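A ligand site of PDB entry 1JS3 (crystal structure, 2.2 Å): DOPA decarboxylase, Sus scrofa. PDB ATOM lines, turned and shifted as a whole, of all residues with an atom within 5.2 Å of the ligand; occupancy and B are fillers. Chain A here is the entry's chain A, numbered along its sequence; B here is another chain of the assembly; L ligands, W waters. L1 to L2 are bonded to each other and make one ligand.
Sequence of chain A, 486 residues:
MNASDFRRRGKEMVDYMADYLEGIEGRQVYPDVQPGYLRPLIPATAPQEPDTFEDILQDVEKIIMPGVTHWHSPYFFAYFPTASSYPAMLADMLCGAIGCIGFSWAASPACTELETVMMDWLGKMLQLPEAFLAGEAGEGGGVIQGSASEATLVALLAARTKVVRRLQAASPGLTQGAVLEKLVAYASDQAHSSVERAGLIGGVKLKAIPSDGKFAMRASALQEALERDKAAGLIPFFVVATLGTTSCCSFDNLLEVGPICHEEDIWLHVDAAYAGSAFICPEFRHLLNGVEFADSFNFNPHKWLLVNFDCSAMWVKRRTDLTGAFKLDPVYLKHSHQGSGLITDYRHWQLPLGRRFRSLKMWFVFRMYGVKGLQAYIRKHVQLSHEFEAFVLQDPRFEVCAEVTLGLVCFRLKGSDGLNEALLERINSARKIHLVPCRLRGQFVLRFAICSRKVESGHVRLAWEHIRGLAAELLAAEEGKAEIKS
The side-chain carboxylate (OD2) of Asp 271 lies within hydrogen-bond range of a nitrogen (N1) of LIG L1 (2.5 Å).
The backbone NH of Ser 149 sits at hydrogen-bond distance from an oxygen (O4) of LIG L1 (2.9 Å).
OG of Ser 149 lies within hydrogen-bond range of O4 of LIG L1, at 2.7 Å.
NZ of Lys 303 lies within salt-bridge range of O5 of LIG L1 (3.9 Å).
The side-chain amide nitrogen of Asn 300 sits at hydrogen-bond distance from an oxygen (O3) of LIG L1 (2.9 Å).
The backbone NH of Ala 148 lies within hydrogen-bond range of an oxygen (O3) of LIG L1.
The backbone carbonyl oxygen (O) of His 302 is in hydrogen-bond range of an oxygen (O1) of LG2 L2 (3.5 Å).
NE2 of His 302 is in hydrogen-bond range of O3 of LIG L1, 2.9 Å away.
OG1 of Thr 82 lies within hydrogen-bond range of O1 of LG2 L2, at 2.9 Å.
The side-chain hydroxyl of Thr 246 is in hydrogen-bond range of an oxygen (O1) of LIG L1 (3.0 Å).
N1 of LG2 L2 lies within hydrogen-bond range of NE2 of His 192 (3.3 Å).
O4 of LIG L1 lies close to OG of Ser 147 (3.5 Å).
N of Ala 273 lies within hydrogen-bond range of OD1 of Asp 271 (3.0 Å).
The side-chain amino group (NZ) of Lys 303 lies close to the side-chain amide nitrogen (ND2) of Asn 300 (3.0 Å).
N of Ala 148 is in hydrogen-bond range of OD1 of Asn 300 (3.4 Å).
ND2 of Asn 300 lies close to NE2 of His 302 (3.4 Å).
The side-chain amide oxygen of Asn 300 lies within hydrogen-bond range of the side-chain hydroxyl of Ser 312 (2.7 Å).
OG of Ser 312 sits at hydrogen-bond distance from N of Ala 148 (3.3 Å).
The backbone carbonyl oxygen of His 302 is in hydrogen-bond range of the side-chain hydroxyl of Thr 82, at 3.2 Å.
The side-chain hydroxyl of Ser 147 is in hydrogen-bond range of the side-chain carboxylate of Glu 150.
Merely in contact with the ligand: Tyr 79 (3.1 Å), Ala 273 (3.5 Å), Pro 81 (3.5 Å), Ser 194 (3.5 Å), Phe 80 (3.6 Å), Ile 101 of chain B (3.7 Å), Phe 103 of chain B (3.7 Å), Trp 71 (3.8 Å), Gly 244 (3.8 Å), Phe 309 (3.9 Å) and Thr 242 (3.99 Å).
Hydrophobic or aromatic side chains that line the ligand: Trp 71, Tyr 79, Phe 80, Ala 148, His 192, Ala 273, His 302, Phe 309, Ile 101 of chain B and Phe 103 of chain B.
21 residues have an atom within 4 Å of the ligand: Trp 71, Tyr 79, Phe 80, Pro 81, Thr 82, Ser 147, Ala 148, Ser 149, His 192, Ser 194, Thr 242, Gly 244, Thr 246, Asp 271, Ala 273, Asn 300, His 302, Lys 303, Phe 309, Ile 101 of chain B and Phe 103 of chain B.
Water W2 lies within hydrogen-bond range of an oxygen (O4) of LIG L1 (2.6 Å), the backbone NH of Leu 353 of chain B (2.7 Å), the backbone NH of Gly 354 of chain B (2.8 Å), the side-chain hydroxyl of Ser 147 (2.9 Å) and the side-chain hydroxyl of Ser 149 (3.3 Å).
Water W4 bridges a ring nitrogen (NE2) of His 192 (3.1 Å) and an oxygen (O4) of LG2 L2 (3.2 Å).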
ATOM      1  N   TRP A  71      17.995  -2.836  25.444  1.00  0.00           N
ATOM      2  CA  TRP A  71      16.958  -2.993  24.435  1.00  0.00           C
ATOM      3  C   TRP A  71      17.268  -2.252  23.146  1.00  0.00           C
ATOM      4  O   TRP A  71      16.804  -2.616  22.072  1.00  0.00           O
ATOM      5  CB  TRP A  71      15.647  -2.429  24.983  1.00  0.00           C
ATOM      6  CG  TRP A  71      14.900  -3.376  25.853  1.00  0.00           C
ATOM      7  CD1 TRP A  71      15.197  -3.720  27.133  1.00  0.00           C
ATOM      8  CD2 TRP A  71      13.744  -4.132  25.488  1.00  0.00           C
ATOM      9  NE1 TRP A  71      14.302  -4.647  27.600  1.00  0.00           N
ATOM     10  CE2 TRP A  71      13.389  -4.919  26.603  1.00  0.00           C
ATOM     11  CE3 TRP A  71      12.965  -4.210  24.320  1.00  0.00           C
ATOM     12  CZ2 TRP A  71      12.291  -5.777  26.594  1.00  0.00           C
ATOM     13  CZ3 TRP A  71      11.877  -5.065  24.310  1.00  0.00           C
ATOM     14  CH2 TRP A  71      11.543  -5.847  25.442  1.00  0.00           C
ATOM     15  N   TYR A  79      12.617 -10.716  21.747  1.00  0.00           N
ATOM     16  CA  TYR A  79      11.211 -10.353  21.804  1.00  0.00           C
ATOM     17  C   TYR A  79      10.762  -9.636  20.555  1.00  0.00           C
ATOM     18  O   TYR A  79      10.747 -10.219  19.466  1.00  0.00           O
ATOM     19  CB  TYR A  79      11.008  -9.426  22.996  1.00  0.00           C
ATOM     20  CG  TYR A  79      11.685  -9.932  24.240  1.00  0.00           C
ATOM     21  CD1 TYR A  79      12.722  -9.225  24.844  1.00  0.00           C
ATOM     22  CD2 TYR A  79      11.317 -11.156  24.811  1.00  0.00           C
ATOM     23  CE1 TYR A  79      13.379  -9.722  25.970  1.00  0.00           C
ATOM     24  CE2 TYR A  79      11.963 -11.656  25.929  1.00  0.00           C
ATOM     25  CZ  TYR A  79      12.991 -10.929  26.504  1.00  0.00           C
ATOM     26  OH  TYR A  79      13.610 -11.404  27.625  1.00  0.00           O
ATOM     27  N   PHE A  80      10.380  -8.386  20.733  1.00  0.00           N
ATOM     28  CA  PHE A  80       9.964  -7.501  19.641  1.00  0.00           C
ATOM     29  C   PHE A  80      10.579  -6.158  20.025  1.00  0.00           C
ATOM     30  O   PHE A  80      10.883  -5.930  21.203  1.00  0.00           O
ATOM     31  CB  PHE A  80       8.434  -7.381  19.575  1.00  0.00           C
ATOM     32  CG  PHE A  80       7.768  -8.400  18.694  1.00  0.00           C
ATOM     33  CD1 PHE A  80       6.495  -8.879  18.994  1.00  0.00           C
ATOM     34  CD2 PHE A  80       8.404  -8.872  17.548  1.00  0.00           C
ATOM     35  CE1 PHE A  80       5.866  -9.798  18.178  1.00  0.00           C
ATOM     36  CE2 PHE A  80       7.774  -9.801  16.712  1.00  0.00           C
ATOM     37  CZ  PHE A  80       6.500 -10.260  17.033  1.00  0.00           C
ATOM     38  N   PRO A  81      10.809  -5.283  19.060  1.00  0.00           N
ATOM     39  CA  PRO A  81      11.384  -3.991  19.439  1.00  0.00           C
ATOM     40  C   PRO A  81      10.506  -3.179  20.377  1.00  0.00           C
ATOM     41  O   PRO A  81       9.289  -3.346  20.386  1.00  0.00           O
ATOM     42  CB  PRO A  81      11.548  -3.274  18.110  1.00  0.00           C
ATOM     43  CG  PRO A  81      10.449  -3.885  17.252  1.00  0.00           C
ATOM     44  CD  PRO A  81      10.587  -5.347  17.597  1.00  0.00           C
ATOM     45  N   THR A  82      11.127  -2.345  21.205  1.00  0.00           N
ATOM     46  CA  THR A  82      10.327  -1.427  22.000  1.00  0.00           C
ATOM     47  C   THR A  82      10.806  -0.113  21.423  1.00  0.00           C
ATOM     48  O   THR A  82      11.927  -0.005  20.943  1.00  0.00           O
ATOM     49  CB  THR A  82      10.546  -1.489  23.514  1.00  0.00           C
ATOM     50  OG1 THR A  82       9.527  -0.690  24.110  1.00  0.00           O
ATOM     51  CG2 THR A  82      11.907  -0.932  23.939  1.00  0.00           C
ATOM     52  N   ALA A  83       9.952   0.901  21.458  1.00  0.00           N
ATOM     53  CA  ALA A  83      10.295   2.162  20.850  1.00  0.00           C
ATOM     54  C   ALA A  83      11.207   3.081  21.604  1.00  0.00           C
ATOM     55  O   ALA A  83      11.105   3.208  22.822  1.00  0.00           O
ATOM     56  CB  ALA A  83       8.999   2.927  20.506  1.00  0.00           C
ATOM     57  N   SER A 147      -1.057   0.098  27.417  1.00  0.00           N
ATOM     58  CA  SER A 147      -0.389  -1.034  26.772  1.00  0.00           C
ATOM     59  C   SER A 147      -1.429  -1.904  26.078  1.00  0.00           C
ATOM     60  O   SER A 147      -2.626  -1.786  26.356  1.00  0.00           O
ATOM     61  CB  SER A 147       0.363  -1.865  27.834  1.00  0.00           C
ATOM     62  OG  SER A 147      -0.548  -2.453  28.768  1.00  0.00           O
ATOM     63  N   ALA A 148      -0.971  -2.790  25.202  1.00  0.00           N
ATOM     64  CA  ALA A 148      -1.883  -3.680  24.498  1.00  0.00           C
ATOM     65  C   ALA A 148      -2.554  -4.654  25.488  1.00  0.00           C
ATOM     66  O   ALA A 148      -3.722  -4.997  25.318  1.00  0.00           O
ATOM     67  CB  ALA A 148      -1.150  -4.460  23.410  1.00  0.00           C
ATOM     68  N   SER A 149      -1.825  -5.078  26.523  1.00  0.00           N
ATOM     69  CA  SER A 149      -2.418  -5.982  27.521  1.00  0.00           C
ATOM     70  C   SER A 149      -3.630  -5.303  28.155  1.00  0.00           C
ATOM     71  O   SER A 149      -4.644  -5.943  28.386  1.00  0.00           O
ATOM     72  CB  SER A 149      -1.418  -6.311  28.647  1.00  0.00           C
ATOM     73  OG  SER A 149      -0.269  -6.958  28.133  1.00  0.00           O
ATOM     74  N   GLU A 150      -3.523  -4.008  28.411  1.00  0.00           N
ATOM     75  CA  GLU A 150      -4.642  -3.265  29.011  1.00  0.00           C
ATOM     76  C   GLU A 150      -5.773  -3.053  27.996  1.00  0.00           C
ATOM     77  O   GLU A 150      -6.939  -3.147  28.331  1.00  0.00           O
ATOM     78  CB  GLU A 150      -4.153  -1.916  29.535  1.00  0.00           C
ATOM     79  CG  GLU A 150      -3.182  -2.069  30.695  1.00  0.00           C
ATOM     80  CD  GLU A 150      -2.458  -0.779  31.022  1.00  0.00           C
ATOM     81  OE1 GLU A 150      -3.012   0.047  31.780  1.00  0.00           O
ATOM     82  OE2 GLU A 150      -1.341  -0.599  30.502  1.00  0.00           O
ATOM     83  N   HIS A 192      -1.070 -13.898  22.473  1.00  0.00           N
ATOM     84  CA  HIS A 192      -0.197 -13.464  23.547  1.00  0.00           C
ATOM     85  C   HIS A 192      -0.840 -13.753  24.906  1.00  0.00           C
ATOM     86  O   HIS A 192      -2.067 -13.771  25.027  1.00  0.00           O
ATOM     87  CB  HIS A 192       0.110 -11.970  23.379  1.00  0.00           C
ATOM     88  CG  HIS A 192       1.151 -11.449  24.326  1.00  0.00           C
ATOM     89  ND1 HIS A 192       0.846 -10.698  25.442  1.00  0.00           N
ATOM     90  CD2 HIS A 192       2.500 -11.591  24.329  1.00  0.00           C
ATOM     91  CE1 HIS A 192       1.952 -10.408  26.087  1.00  0.00           C
ATOM     92  NE2 HIS A 192       2.977 -10.935  25.430  1.00  0.00           N
ATOM     93  N   SER A 194      -1.308 -11.978  27.360  1.00  0.00           N
ATOM     94  CA  SER A 194      -2.151 -10.905  27.848  1.00  0.00           C
ATOM     95  C   SER A 194      -3.641 -11.234  27.644  1.00  0.00           C
ATOM     96  O   SER A 194      -4.502 -10.709  28.348  1.00  0.00           O
ATOM     97  CB  SER A 194      -1.806  -9.599  27.129  1.00  0.00           C
ATOM     98  OG  SER A 194      -1.809  -9.786  25.734  1.00  0.00           O
ATOM     99  N   THR A 242      -5.315 -12.116  16.338  1.00  0.00           N
ATOM    100  CA  THR A 242      -3.974 -11.574  16.463  1.00  0.00           C
ATOM    101  C   THR A 242      -3.315 -11.393  15.101  1.00  0.00           C
ATOM    102  O   THR A 242      -3.265 -12.320  14.286  1.00  0.00           O
ATOM    103  CB  THR A 242      -3.069 -12.483  17.300  1.00  0.00           C
ATOM    104  OG1 THR A 242      -3.652 -12.724  18.579  1.00  0.00           O
ATOM    105  CG2 THR A 242      -1.716 -11.827  17.493  1.00  0.00           C
ATOM    106  N   GLY A 244       0.211 -10.643  13.810  1.00  0.00           N
ATOM    107  CA  GLY A 244       1.600 -10.501  14.211  1.00  0.00           C
ATOM    108  C   GLY A 244       1.854 -11.186  15.538  1.00  0.00           C
ATOM    109  O   GLY A 244       2.232 -10.531  16.523  1.00  0.00           O
ATOM    110  N   THR A 245       1.648 -12.496  15.579  1.00  0.00           N
ATOM    111  CA  THR A 245       1.850 -13.283  16.793  1.00  0.00           C
ATOM    112  C   THR A 245       3.296 -13.212  17.256  1.00  0.00           C
ATOM    113  O   THR A 245       4.224 -13.067  16.452  1.00  0.00           O
ATOM    114  CB  THR A 245       1.467 -14.751  16.568  1.00  0.00           C
ATOM    115  OG1 THR A 245       2.311 -15.310  15.554  1.00  0.00           O
ATOM    116  CG2 THR A 245       0.004 -14.868  16.128  1.00  0.00           C
ATOM    117  N   THR A 246       3.486 -13.325  18.553  1.00  0.00           N
ATOM    118  CA  THR A 246       4.799 -13.250  19.177  1.00  0.00           C
ATOM    119  C   THR A 246       5.755 -14.350  18.763  1.00  0.00           C
ATOM    120  O   THR A 246       6.935 -14.102  18.507  1.00  0.00           O
ATOM    121  CB  THR A 246       4.658 -13.278  20.704  1.00  0.00           C
ATOM    122  OG1 THR A 246       3.713 -12.268  21.106  1.00  0.00           O
ATOM    123  CG2 THR A 246       5.968 -12.959  21.369  1.00  0.00           C
ATOM    124  N   ASP A 271      -5.826  -7.673  17.968  1.00  0.00           N
ATOM    125  CA  ASP A 271      -4.556  -7.405  18.629  1.00  0.00           C
ATOM    126  C   ASP A 271      -3.451  -7.414  17.566  1.00  0.00           C
ATOM    127  O   ASP A 271      -3.113  -8.465  17.011  1.00  0.00           O
ATOM    128  CB  ASP A 271      -4.286  -8.469  19.702  1.00  0.00           C
ATOM    129  CG  ASP A 271      -2.888  -8.363  20.313  1.00  0.00           C
ATOM    130  OD1 ASP A 271      -2.141  -7.425  19.990  1.00  0.00           O
ATOM    131  OD2 ASP A 271      -2.517  -9.229  21.138  1.00  0.00           O
ATOM    132  N   ALA A 273      -0.454  -5.708  18.192  1.00  0.00           N
ATOM    133  CA  ALA A 273       0.584  -5.027  18.968  1.00  0.00           C
ATOM    134  C   ALA A 273       1.829  -4.641  18.187  1.00  0.00           C
ATOM    135  O   ALA A 273       2.173  -3.460  18.084  1.00  0.00           O
ATOM    136  CB  ALA A 273       0.965  -5.873  20.175  1.00  0.00           C
ATOM    137  N   TYR A 274       2.506  -5.629  17.632  1.00  0.00           N
ATOM    138  CA  TYR A 274       3.728  -5.383  16.874  1.00  0.00           C
ATOM    139  C   TYR A 274       3.483  -5.030  15.404  1.00  0.00           C
ATOM    140  O   TYR A 274       3.842  -3.946  14.956  1.00  0.00           O
ATOM    141  CB  TYR A 274       4.650  -6.601  16.951  1.00  0.00           C
ATOM    142  CG  TYR A 274       5.790  -6.593  15.943  1.00  0.00           C
ATOM    143  CD1 TYR A 274       6.852  -5.687  16.068  1.00  0.00           C
ATOM    144  CD2 TYR A 274       5.806  -7.489  14.879  1.00  0.00           C
ATOM    145  CE1 TYR A 274       7.915  -5.691  15.152  1.00  0.00           C
ATOM    146  CE2 TYR A 274       6.858  -7.496  13.955  1.00  0.00           C
ATOM    147  CZ  TYR A 274       7.902  -6.594  14.093  1.00  0.00           C
ATOM    148  OH  TYR A 274       8.946  -6.603  13.180  1.00  0.00           O
ATOM    149  N   ASN A 300       0.597  -1.350  19.115  1.00  0.00           N
ATOM    150  CA  ASN A 300       1.468  -0.526  19.926  1.00  0.00           C
ATOM    151  C   ASN A 300       2.451   0.370  19.224  1.00  0.00           C
ATOM    152  O   ASN A 300       3.431  -0.099  18.644  1.00  0.00           O
ATOM    153  CB  ASN A 300       2.294  -1.368  20.906  1.00  0.00           C
ATOM    154  CG  ASN A 300       1.464  -2.043  21.959  1.00  0.00           C
ATOM    155  OD1 ASN A 300       0.429  -1.530  22.385  1.00  0.00           O
ATOM    156  ND2 ASN A 300       1.926  -3.202  22.407  1.00  0.00           N
ATOM    157  N   HIS A 302       4.315   1.951  20.706  1.00  0.00           N
ATOM    158  CA  HIS A 302       5.486   1.817  21.563  1.00  0.00           C
ATOM    159  C   HIS A 302       6.312   0.577  21.300  1.00  0.00           C
ATOM    160  O   HIS A 302       7.282   0.285  22.006  1.00  0.00           O
ATOM    161  CB  HIS A 302       5.173   1.995  23.055  1.00  0.00           C
ATOM    162  CG  HIS A 302       4.338   0.912  23.665  1.00  0.00           C
ATOM    163  ND1 HIS A 302       3.393   1.181  24.634  1.00  0.00           N
ATOM    164  CD2 HIS A 302       4.375  -0.434  23.529  1.00  0.00           C
ATOM    165  CE1 HIS A 302       2.880   0.039  25.064  1.00  0.00           C
ATOM    166  NE2 HIS A 302       3.461  -0.959  24.412  1.00  0.00           N
ATOM    167  N   LYS A 303       5.946  -0.156  20.263  1.00  0.00           N
ATOM    168  CA  LYS A 303       6.765  -1.280  19.869  1.00  0.00           C
ATOM    169  C   LYS A 303       7.517  -0.864  18.625  1.00  0.00           C
ATOM    170  O   LYS A 303       8.715  -0.582  18.680  1.00  0.00           O
ATOM    171  CB  LYS A 303       5.943  -2.521  19.527  1.00  0.00           C
ATOM    172  CG  LYS A 303       5.736  -3.449  20.700  1.00  0.00           C
ATOM    173  CD  LYS A 303       5.223  -4.764  20.211  1.00  0.00           C
ATOM    174  CE  LYS A 303       5.084  -5.684  21.364  1.00  0.00           C
ATOM    175  NZ  LYS A 303       4.308  -4.987  22.439  1.00  0.00           N
ATOM    176  N   PHE A 309       7.618   3.816  24.997  1.00  0.00           N
ATOM    177  CA  PHE A 309       6.653   3.126  25.817  1.00  0.00           C
ATOM    178  C   PHE A 309       5.928   3.996  26.763  1.00  0.00           C
ATOM    179  O   PHE A 309       6.483   4.850  27.459  1.00  0.00           O
ATOM    180  CB  PHE A 309       7.248   1.967  26.599  1.00  0.00           C
ATOM    181  CG  PHE A 309       6.244   1.265  27.487  1.00  0.00           C
ATOM    182  CD1 PHE A 309       6.067   1.669  28.806  1.00  0.00           C
ATOM    183  CD2 PHE A 309       5.511   0.174  27.019  1.00  0.00           C
ATOM    184  CE1 PHE A 309       5.171   0.974  29.667  1.00  0.00           C
ATOM    185  CE2 PHE A 309       4.621  -0.518  27.849  1.00  0.00           C
ATOM    186  CZ  PHE A 309       4.457  -0.112  29.188  1.00  0.00           C
ATOM    187  N   SER A 312      -0.055   2.757  23.658  1.00  0.00           N
ATOM    188  CA  SER A 312      -0.756   1.714  22.923  1.00  0.00           C
ATOM    189  C   SER A 312      -1.959   2.440  22.292  1.00  0.00           C
ATOM    190  O   SER A 312      -2.612   3.266  22.945  1.00  0.00           O
ATOM    191  CB  SER A 312      -1.224   0.617  23.873  1.00  0.00           C
ATOM    192  OG  SER A 312      -1.875  -0.414  23.141  1.00  0.00           O
ATOM    193  N   ILE B 101      11.648  -2.442  28.902  1.00  0.00           N
ATOM    194  CA  ILE B 101      10.280  -2.824  29.287  1.00  0.00           C
ATOM    195  C   ILE B 101      10.507  -3.949  30.315  1.00  0.00           C
ATOM    196  O   ILE B 101      10.816  -5.074  29.926  1.00  0.00           O
ATOM    197  CB  ILE B 101       9.450  -3.367  28.106  1.00  0.00           C
ATOM    198  CG1 ILE B 101       9.430  -2.352  26.956  1.00  0.00           C
ATOM    199  CG2 ILE B 101       8.026  -3.642  28.580  1.00  0.00           C
ATOM    200  CD1 ILE B 101       9.030  -0.971  27.378  1.00  0.00           C
ATOM    201  N   PHE B 103       9.109  -6.338  31.868  1.00  0.00           N
ATOM    202  CA  PHE B 103       8.063  -7.333  32.044  1.00  0.00           C
ATOM    203  C   PHE B 103       8.583  -8.609  32.685  1.00  0.00           C
ATOM    204  O   PHE B 103       7.826  -9.489  33.041  1.00  0.00           O
ATOM    205  CB  PHE B 103       7.395  -7.625  30.697  1.00  0.00           C
ATOM    206  CG  PHE B 103       8.330  -8.150  29.649  1.00  0.00           C
ATOM    207  CD1 PHE B 103       8.721  -9.487  29.663  1.00  0.00           C
ATOM    208  CD2 PHE B 103       8.848  -7.307  28.672  1.00  0.00           C
ATOM    209  CE1 PHE B 103       9.616  -9.964  28.712  1.00  0.00           C
ATOM    210  CE2 PHE B 103       9.745  -7.784  27.731  1.00  0.00           C
ATOM    211  CZ  PHE B 103      10.136  -9.121  27.745  1.00  0.00           C
ATOM    212  N   LEU B 353       1.383  -5.967  31.679  1.00  0.00           N
ATOM    213  CA  LEU B 353       2.518  -6.861  31.632  1.00  0.00           C
ATOM    214  C   LEU B 353       3.787  -6.030  31.555  1.00  0.00           C
ATOM    215  O   LEU B 353       4.756  -6.271  32.271  1.00  0.00           O
ATOM    216  CB  LEU B 353       2.368  -7.771  30.411  1.00  0.00           C
ATOM    217  CG  LEU B 353       2.267  -9.287  30.599  1.00  0.00           C
ATOM    218  CD1 LEU B 353       1.767  -9.635  31.978  1.00  0.00           C
ATOM    219  CD2 LEU B 353       1.352  -9.854  29.512  1.00  0.00           C
ATOM    220  N   GLY B 354       3.779  -5.022  30.686  1.00  0.00           N
ATOM    221  CA  GLY B 354       4.938  -4.164  30.544  1.00  0.00           C
ATOM    222  C   GLY B 354       4.991  -3.109  31.637  1.00  0.00           C
ATOM    223  O   GLY B 354       4.051  -2.945  32.393  1.00  0.00           O
HETATM  224  N1  LIG L   1      -0.197  -8.738  21.947  1.00  0.00           N
HETATM  225  C1  LIG L   1       0.916  -9.161  21.286  1.00  0.00           C
HETATM  226  C2  LIG L   1       0.752  -9.907  19.967  1.00  0.00           C
HETATM  227  C3  LIG L   1       2.182  -8.910  21.817  1.00  0.00           C
HETATM  228  O1  LIG L   1       3.305  -9.268  21.125  1.00  0.00           O
HETATM  229  C4  LIG L   1       2.285  -8.237  23.024  1.00  0.00           C
HETATM  230  C5  LIG L   1       3.578  -7.561  23.408  1.00  0.00           C
HETATM  231  C6  LIG L   1       1.127  -7.845  23.681  1.00  0.00           C
HETATM  232  C7  LIG L   1      -0.089  -8.094  23.133  1.00  0.00           C
HETATM  233  C8  LIG L   1       1.210  -7.005  24.962  1.00  0.00           C
HETATM  234  O2  LIG L   1       1.617  -5.667  24.638  1.00  0.00           O
HETATM  235  P1  LIG L   1       2.114  -4.658  25.767  1.00  0.00           P
HETATM  236  O3  LIG L   1       1.881  -3.285  25.265  1.00  0.00           O
HETATM  237  O4  LIG L   1       1.084  -4.954  26.961  1.00  0.00           O
HETATM  238  O5  LIG L   1       3.467  -5.051  26.213  1.00  0.00           O
HETATM  239  N1  LG2 L   2       5.340  -9.187  23.957  1.00  0.00           N
HETATM  240  N2  LG2 L   2       4.826  -7.865  23.790  1.00  0.00           N
HETATM  241  C1  LG2 L   2       6.613  -9.244  23.940  1.00  0.00           C
HETATM  242  C2  LG2 L   2       7.286  -8.259  24.952  1.00  0.00           C
HETATM  243  C3  LG2 L   2       7.115  -8.926  22.531  1.00  0.00           C
HETATM  244  C4  LG2 L   2       7.307  -6.758  24.624  1.00  0.00           C
HETATM  245  C5  LG2 L   2       6.456  -5.879  25.296  1.00  0.00           C
HETATM  246  C6  LG2 L   2       6.458  -4.499  25.052  1.00  0.00           C
HETATM  247  C7  LG2 L   2       8.186  -6.209  23.685  1.00  0.00           C
HETATM  248  C8  LG2 L   2       8.200  -4.805  23.419  1.00  0.00           C
HETATM  249  C9  LG2 L   2       7.322  -3.965  24.125  1.00  0.00           C
HETATM  250  O1  LG2 L   2       7.290  -2.595  23.917  1.00  0.00           O
HETATM  251  O2  LG2 L   2       5.612  -3.640  25.723  1.00  0.00           O
HETATM  252  C10 LG2 L   2       7.043 -10.668  24.352  1.00  0.00           C
HETATM  253  O3  LG2 L   2       8.276 -10.880  24.372  1.00  0.00           O
HETATM  254  O4  LG2 L   2       6.294 -11.213  25.192  1.00  0.00           O
HETATM  255  O   HOH W   1       4.338  -6.923  27.784  1.00  0.00           O
HETATM  256  O   HOH W   2       1.373  -4.458  29.465  1.00  0.00           O
HETATM  257  O   HOH W   3       8.381 -12.904  26.349  1.00  0.00           O
HETATM  258  O   HOH W   4       4.831  -9.211  27.156  1.00  0.00           O
HETATM  259  O   HOH W   5       8.620 -13.011  22.654  1.00  0.00           O
